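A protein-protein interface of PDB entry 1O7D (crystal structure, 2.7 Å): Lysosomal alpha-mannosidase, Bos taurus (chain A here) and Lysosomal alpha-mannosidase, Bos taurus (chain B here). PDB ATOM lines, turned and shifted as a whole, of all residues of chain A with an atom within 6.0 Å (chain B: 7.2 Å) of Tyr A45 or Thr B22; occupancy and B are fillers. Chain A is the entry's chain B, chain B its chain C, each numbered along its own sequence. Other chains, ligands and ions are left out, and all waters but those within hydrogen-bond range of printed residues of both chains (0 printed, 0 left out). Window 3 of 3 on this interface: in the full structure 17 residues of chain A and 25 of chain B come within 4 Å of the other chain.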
ATOM      1  N   PHE A  32      25.345 -19.802 -18.552  1.00  0.00           N
ATOM      2  CA  PHE A  32      25.238 -18.411 -18.204  1.00  0.00           C
ATOM      3  C   PHE A  32      24.986 -18.417 -16.751  1.00  0.00           C
ATOM      4  O   PHE A  32      24.283 -19.288 -16.247  1.00  0.00           O
ATOM      5  CB  PHE A  32      24.097 -17.810 -18.957  1.00  0.00           C
ATOM      6  CG  PHE A  32      24.509 -17.610 -20.434  1.00  0.00           C
ATOM      7  CD1 PHE A  32      25.482 -16.635 -20.824  1.00  0.00           C
ATOM      8  CD2 PHE A  32      23.956 -18.400 -21.435  1.00  0.00           C
ATOM      9  CE1 PHE A  32      25.854 -16.501 -22.216  1.00  0.00           C
ATOM     10  CE2 PHE A  32      24.313 -18.271 -22.767  1.00  0.00           C
ATOM     11  CZ  PHE A  32      25.230 -17.319 -23.152  1.00  0.00           C
ATOM     12  N   TRP A  42      30.390 -11.170 -17.201  1.00  0.00           N
ATOM     13  CA  TRP A  42      30.309 -10.764 -18.581  1.00  0.00           C
ATOM     14  C   TRP A  42      28.838 -10.723 -18.954  1.00  0.00           C
ATOM     15  O   TRP A  42      28.424 -11.340 -19.917  1.00  0.00           O
ATOM     16  CB  TRP A  42      31.074 -11.756 -19.453  1.00  0.00           C
ATOM     17  CG  TRP A  42      32.571 -11.745 -19.218  1.00  0.00           C
ATOM     18  CD1 TRP A  42      33.237 -11.831 -18.011  1.00  0.00           C
ATOM     19  CD2 TRP A  42      33.579 -11.724 -20.226  1.00  0.00           C
ATOM     20  NE1 TRP A  42      34.596 -11.872 -18.225  1.00  0.00           N
ATOM     21  CE2 TRP A  42      34.832 -11.809 -19.574  1.00  0.00           C
ATOM     22  CE3 TRP A  42      33.546 -11.645 -21.623  1.00  0.00           C
ATOM     23  CZ2 TRP A  42      36.040 -11.817 -20.282  1.00  0.00           C
ATOM     24  CZ3 TRP A  42      34.746 -11.654 -22.323  1.00  0.00           C
ATOM     25  CH2 TRP A  42      35.975 -11.740 -21.651  1.00  0.00           C
ATOM     26  N   THR A  43      28.047  -9.993 -18.183  1.00  0.00           N
ATOM     27  CA  THR A  43      26.630  -9.897 -18.469  1.00  0.00           C
ATOM     28  C   THR A  43      26.204  -8.528 -19.006  1.00  0.00           C
ATOM     29  O   THR A  43      25.025  -8.288 -19.256  1.00  0.00           O
ATOM     30  CB  THR A  43      25.803 -10.231 -17.216  1.00  0.00           C
ATOM     31  OG1 THR A  43      26.099  -9.290 -16.177  1.00  0.00           O
ATOM     32  CG2 THR A  43      26.138 -11.640 -16.737  1.00  0.00           C
ATOM     33  N   GLY A  44      27.172  -7.644 -19.209  1.00  0.00           N
ATOM     34  CA  GLY A  44      26.857  -6.314 -19.700  1.00  0.00           C
ATOM     35  C   GLY A  44      26.686  -6.212 -21.204  1.00  0.00           C
ATOM     36  O   GLY A  44      25.995  -5.309 -21.694  1.00  0.00           O
ATOM     37  N   TYR A  45      27.305  -7.128 -21.945  1.00  0.00           N
ATOM     38  CA  TYR A  45      27.196  -7.097 -23.397  1.00  0.00           C
ATOM     39  C   TYR A  45      25.855  -7.650 -23.862  1.00  0.00           C
ATOM     40  O   TYR A  45      25.568  -7.674 -25.061  1.00  0.00           O
ATOM     41  CB  TYR A  45      28.336  -7.884 -24.052  1.00  0.00           C
ATOM     42  CG  TYR A  45      28.212  -9.394 -23.985  1.00  0.00           C
ATOM     43  CD1 TYR A  45      28.539 -10.093 -22.826  1.00  0.00           C
ATOM     44  CD2 TYR A  45      27.781 -10.125 -25.093  1.00  0.00           C
ATOM     45  CE1 TYR A  45      28.441 -11.486 -22.769  1.00  0.00           C
ATOM     46  CE2 TYR A  45      27.679 -11.512 -25.047  1.00  0.00           C
ATOM     47  CZ  TYR A  45      28.010 -12.187 -23.878  1.00  0.00           C
ATOM     48  OH  TYR A  45      27.895 -13.560 -23.815  1.00  0.00           O
ATOM     49  N   PHE A  46      25.036  -8.106 -22.921  1.00  0.00           N
ATOM     50  CA  PHE A  46      23.736  -8.633 -23.284  1.00  0.00           C
ATOM     51  C   PHE A  46      22.891  -7.499 -23.823  1.00  0.00           C
ATOM     52  O   PHE A  46      21.927  -7.721 -24.546  1.00  0.00           O
ATOM     53  CB  PHE A  46      23.047  -9.269 -22.082  1.00  0.00           C
ATOM     54  CG  PHE A  46      23.724 -10.519 -21.585  1.00  0.00           C
ATOM     55  CD1 PHE A  46      24.567 -11.249 -22.415  1.00  0.00           C
ATOM     56  CD2 PHE A  46      23.495 -10.977 -20.288  1.00  0.00           C
ATOM     57  CE1 PHE A  46      25.173 -12.403 -21.967  1.00  0.00           C
ATOM     58  CE2 PHE A  46      24.100 -12.135 -19.831  1.00  0.00           C
ATOM     59  CZ  PHE A  46      24.938 -12.848 -20.672  1.00  0.00           C
ATOM     60  N   SER A  47      23.273  -6.273 -23.482  1.00  0.00           N
ATOM     61  CA  SER A  47      22.540  -5.105 -23.928  1.00  0.00           C
ATOM     62  C   SER A  47      23.439  -4.072 -24.565  1.00  0.00           C
ATOM     63  O   SER A  47      22.959  -3.101 -25.119  1.00  0.00           O
ATOM     64  CB  SER A  47      21.793  -4.481 -22.756  1.00  0.00           C
ATOM     65  OG  SER A  47      20.822  -5.385 -22.272  1.00  0.00           O
ATOM     66  N   SER A  48      24.744  -4.268 -24.499  1.00  0.00           N
ATOM     67  CA  SER A  48      25.650  -3.306 -25.098  1.00  0.00           C
ATOM     68  C   SER A  48      25.290  -3.014 -26.559  1.00  0.00           C
ATOM     69  O   SER A  48      24.984  -3.931 -27.332  1.00  0.00           O
ATOM     70  CB  SER A  48      27.082  -3.822 -25.009  1.00  0.00           C
ATOM     71  OG  SER A  48      27.445  -4.036 -23.662  1.00  0.00           O
ATOM     72  N   ARG A  49      25.324  -1.731 -26.927  1.00  0.00           N
ATOM     73  CA  ARG A  49      25.024  -1.288 -28.296  1.00  0.00           C
ATOM     74  C   ARG A  49      23.620  -1.660 -28.810  1.00  0.00           C
ATOM     75  O   ARG A  49      23.483  -2.400 -29.784  1.00  0.00           O
ATOM     76  CB  ARG A  49      26.067  -1.844 -29.280  1.00  0.00           C
ATOM     77  CG  ARG A  49      27.473  -1.330 -29.090  1.00  0.00           C
ATOM     78  CD  ARG A  49      28.357  -1.715 -30.263  1.00  0.00           C
ATOM     79  NE  ARG A  49      29.740  -1.274 -30.081  1.00  0.00           N
ATOM     80  CZ  ARG A  49      30.149  -0.006 -30.137  1.00  0.00           C
ATOM     81  NH1 ARG A  49      29.286   0.969 -30.380  1.00  0.00           N
ATOM     82  NH2 ARG A  49      31.425   0.293 -29.935  1.00  0.00           N
ATOM     83  N   LYS A  53      22.382  -3.849 -32.270  1.00  0.00           N
ATOM     84  CA  LYS A  53      21.677  -5.082 -31.973  1.00  0.00           C
ATOM     85  C   LYS A  53      20.340  -5.136 -32.709  1.00  0.00           C
ATOM     86  O   LYS A  53      19.992  -6.161 -33.282  1.00  0.00           O
ATOM     87  CB  LYS A  53      21.488  -5.237 -30.460  1.00  0.00           C
ATOM     88  CG  LYS A  53      22.639  -5.970 -29.766  1.00  0.00           C
ATOM     89  CD  LYS A  53      22.535  -5.911 -28.235  1.00  0.00           C
ATOM     90  CE  LYS A  53      23.499  -6.885 -27.533  1.00  0.00           C
ATOM     91  NZ  LYS A  53      24.933  -6.520 -27.635  1.00  0.00           N
ATOM     92  N   HIS B  15      29.454 -12.626 -35.664  1.00  0.00           N
ATOM     93  CA  HIS B  15      30.720 -12.818 -34.953  1.00  0.00           C
ATOM     94  C   HIS B  15      30.496 -12.606 -33.446  1.00  0.00           C
ATOM     95  O   HIS B  15      29.426 -12.143 -33.040  1.00  0.00           O
ATOM     96  CB  HIS B  15      31.734 -11.801 -35.468  1.00  0.00           C
ATOM     97  CG  HIS B  15      33.087 -11.922 -34.810  1.00  0.00           C
ATOM     98  ND1 HIS B  15      33.892 -13.025 -34.971  1.00  0.00           N
ATOM     99  CD2 HIS B  15      33.734 -11.080 -33.978  1.00  0.00           C
ATOM    100  CE1 HIS B  15      34.999 -12.853 -34.254  1.00  0.00           C
ATOM    101  NE2 HIS B  15      34.929 -11.692 -33.647  1.00  0.00           N
ATOM    102  N   HIS B  16      31.510 -12.910 -32.633  1.00  0.00           N
ATOM    103  CA  HIS B  16      31.359 -12.738 -31.181  1.00  0.00           C
ATOM    104  C   HIS B  16      31.763 -11.368 -30.641  1.00  0.00           C
ATOM    105  O   HIS B  16      31.544 -11.065 -29.473  1.00  0.00           O
ATOM    106  CB  HIS B  16      32.087 -13.834 -30.411  1.00  0.00           C
ATOM    107  CG  HIS B  16      33.539 -13.999 -30.801  1.00  0.00           C
ATOM    108  ND1 HIS B  16      33.941 -14.792 -31.845  1.00  0.00           N
ATOM    109  CD2 HIS B  16      34.654 -13.511 -30.217  1.00  0.00           C
ATOM    110  CE1 HIS B  16      35.273 -14.800 -31.884  1.00  0.00           C
ATOM    111  NE2 HIS B  16      35.720 -14.042 -30.915  1.00  0.00           N
ATOM    112  N   ASP B  17      32.328 -10.541 -31.506  1.00  0.00           N
ATOM    113  CA  ASP B  17      32.727  -9.209 -31.125  1.00  0.00           C
ATOM    114  C   ASP B  17      31.854  -8.207 -31.850  1.00  0.00           C
ATOM    115  O   ASP B  17      32.009  -7.004 -31.647  1.00  0.00           O
ATOM    116  CB  ASP B  17      34.178  -8.927 -31.522  1.00  0.00           C
ATOM    117  CG  ASP B  17      35.162  -9.780 -30.787  1.00  0.00           C
ATOM    118  OD1 ASP B  17      34.870 -10.082 -29.611  1.00  0.00           O
ATOM    119  OD2 ASP B  17      36.223 -10.126 -31.373  1.00  0.00           O
ATOM    120  N   ALA B  18      30.958  -8.687 -32.708  1.00  0.00           N
ATOM    121  CA  ALA B  18      30.080  -7.787 -33.471  1.00  0.00           C
ATOM    122  C   ALA B  18      28.744  -7.415 -32.805  1.00  0.00           C
ATOM    123  O   ALA B  18      28.631  -6.366 -32.188  1.00  0.00           O
ATOM    124  CB  ALA B  18      29.827  -8.375 -34.882  1.00  0.00           C
ATOM    125  N   VAL B  19      27.743  -8.280 -32.941  1.00  0.00           N
ATOM    126  CA  VAL B  19      26.427  -8.053 -32.373  1.00  0.00           C
ATOM    127  C   VAL B  19      26.510  -7.925 -30.868  1.00  0.00           C
ATOM    128  O   VAL B  19      25.673  -7.268 -30.267  1.00  0.00           O
ATOM    129  CB  VAL B  19      25.466  -9.204 -32.725  1.00  0.00           C
ATOM    130  CG1 VAL B  19      25.931 -10.509 -32.066  1.00  0.00           C
ATOM    131  CG2 VAL B  19      24.080  -8.870 -32.247  1.00  0.00           C
ATOM    132  N   SER B  20      27.499  -8.568 -30.258  1.00  0.00           N
ATOM    133  CA  SER B  20      27.701  -8.513 -28.808  1.00  0.00           C
ATOM    134  C   SER B  20      28.122  -7.076 -28.444  1.00  0.00           C
ATOM    135  O   SER B  20      28.114  -6.680 -27.273  1.00  0.00           O
ATOM    136  CB  SER B  20      28.788  -9.517 -28.420  1.00  0.00           C
ATOM    137  OG  SER B  20      29.892  -9.383 -29.297  1.00  0.00           O
ATOM    138  N   GLY B  21      28.480  -6.311 -29.478  1.00  0.00           N
ATOM    139  CA  GLY B  21      28.897  -4.928 -29.318  1.00  0.00           C
ATOM    140  C   GLY B  21      30.205  -4.804 -28.582  1.00  0.00           C
ATOM    141  O   GLY B  21      30.467  -3.787 -27.946  1.00  0.00           O
ATOM    142  N   THR B  22      31.037  -5.831 -28.678  1.00  0.00           N
ATOM    143  CA  THR B  22      32.305  -5.817 -27.977  1.00  0.00           C
ATOM    144  C   THR B  22      33.490  -5.475 -28.843  1.00  0.00           C
ATOM    145  O   THR B  22      34.610  -5.890 -28.574  1.00  0.00           O
ATOM    146  CB  THR B  22      32.555  -7.154 -27.269  1.00  0.00           C
ATOM    147  OG1 THR B  22      32.520  -8.232 -28.217  1.00  0.00           O
ATOM    148  CG2 THR B  22      31.505  -7.359 -26.193  1.00  0.00           C
ATOM    149  N   SER B  23      33.248  -4.696 -29.882  1.00  0.00           N
ATOM    150  CA  SER B  23      34.328  -4.291 -30.764  1.00  0.00           C
ATOM    151  C   SER B  23      34.489  -2.782 -30.664  1.00  0.00           C
ATOM    152  O   SER B  23      33.649  -2.092 -30.085  1.00  0.00           O
ATOM    153  CB  SER B  23      34.016  -4.694 -32.205  1.00  0.00           C
ATOM    154  OG  SER B  23      32.756  -4.181 -32.604  1.00  0.00           O
ATOM    155  N   ARG B  24      35.580  -2.280 -31.223  1.00  0.00           N
ATOM    156  CA  ARG B  24      35.834  -0.859 -31.211  1.00  0.00           C
ATOM    157  C   ARG B  24      34.829  -0.118 -32.086  1.00  0.00           C
ATOM    158  O   ARG B  24      34.195  -0.708 -32.976  1.00  0.00           O
ATOM    159  CB  ARG B  24      37.263  -0.575 -31.668  1.00  0.00           C
ATOM    160  CG  ARG B  24      38.267  -0.829 -30.574  1.00  0.00           C
ATOM    161  CD  ARG B  24      39.643  -0.359 -30.930  1.00  0.00           C
ATOM    162  NE  ARG B  24      40.465  -0.292 -29.732  1.00  0.00           N
ATOM    163  CZ  ARG B  24      41.754   0.035 -29.728  1.00  0.00           C
ATOM    164  NH1 ARG B  24      42.365   0.320 -30.869  1.00  0.00           N
ATOM    165  NH2 ARG B  24      42.430   0.093 -28.586  1.00  0.00           N
ATOM    166  N   TYR B  31      30.657  -2.384 -39.418  1.00  0.00           N
ATOM    167  CA  TYR B  31      29.735  -3.513 -39.370  1.00  0.00           C
ATOM    168  C   TYR B  31      28.412  -3.049 -39.950  1.00  0.00           C
ATOM    169  O   TYR B  31      27.834  -3.704 -40.829  1.00  0.00           O
ATOM    170  CB  TYR B  31      29.506  -4.003 -37.941  1.00  0.00           C
ATOM    171  CG  TYR B  31      30.558  -4.955 -37.410  1.00  0.00           C
ATOM    172  CD1 TYR B  31      31.099  -5.952 -38.219  1.00  0.00           C
ATOM    173  CD2 TYR B  31      30.988  -4.877 -36.083  1.00  0.00           C
ATOM    174  CE1 TYR B  31      32.047  -6.851 -37.716  1.00  0.00           C
ATOM    175  CE2 TYR B  31      31.931  -5.771 -35.568  1.00  0.00           C
ATOM    176  CZ  TYR B  31      32.458  -6.756 -36.390  1.00  0.00           C
ATOM    177  OH  TYR B  31      33.386  -7.644 -35.894  1.00  0.00           O
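The side-chain hydroxyl of Thr B22 is in hydrogen-bond range of the side-chain hydroxyl of Ser B20 (3.1 Å).
O of Ser A48 is in hydrogen-bond range of NZ of Lys A53, 2.6 Å away.
OG of Ser A48 lies within hydrogen-bond range of O of Gly A44, 2.8 Å away.
NZ of Lys A53 lies within hydrogen-bond range of O of Tyr A45, 2.9 Å away.
The side-chain hydroxyl (OG) of Ser B20 sits close to the backbone NH (N) of Asp B17, at 3.5 Å.
The side-chain hydroxyl (OG1) of Thr B22 lies close to the side-chain carboxylate (OD1) of Asp B17, at 3.3 Å.
CB of Tyr A45 touches O of Ser B20 (3.4 Å).
Tyr A45 touches Thr B22 (CB to CG2, 3.9 Å).
Ser A48 touches Ser B20.
Of the 11 printed residues of chain B, 5 touch a printed residue of chain A.
The side-chain amino group of Lys A53 lies within hydrogen-bond range of the backbone carbonyl oxygen of Val B19, at 2.8 Å.
O of Ser B23 lies within hydrogen-bond range of NH2 of Arg A49 (3.3 Å).
The guanidinium group of Arg A49 is in hydrogen-bond range of the backbone carbonyl oxygen of Gly B21 (3.4 Å).
The side-chain amino group (NZ) of Lys A53 is in hydrogen-bond range of the backbone carbonyl oxygen (O) of Ser B20 (3.2 Å).
Thr B22 touches just one residue of chain A: Tyr A45.
No residue of chain B comes within 4 Å of Gly A44.
Printed residues of chain B within 4 Å of Ser A48: Ser B20.
Of the printed residues of chain A, Ser B23 touches Arg A49 (3.3 Å).
His B15 touches none of the printed residues of chain A.
Phe A46 touches none of the printed residues of chain B.
The nearest residue of chain B that does not touch Tyr A45 is Val B19 (5.2 Å).
The nearest printed residue of chain A that does not touch Ser B23 is Ser A48 (7.9 Å).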
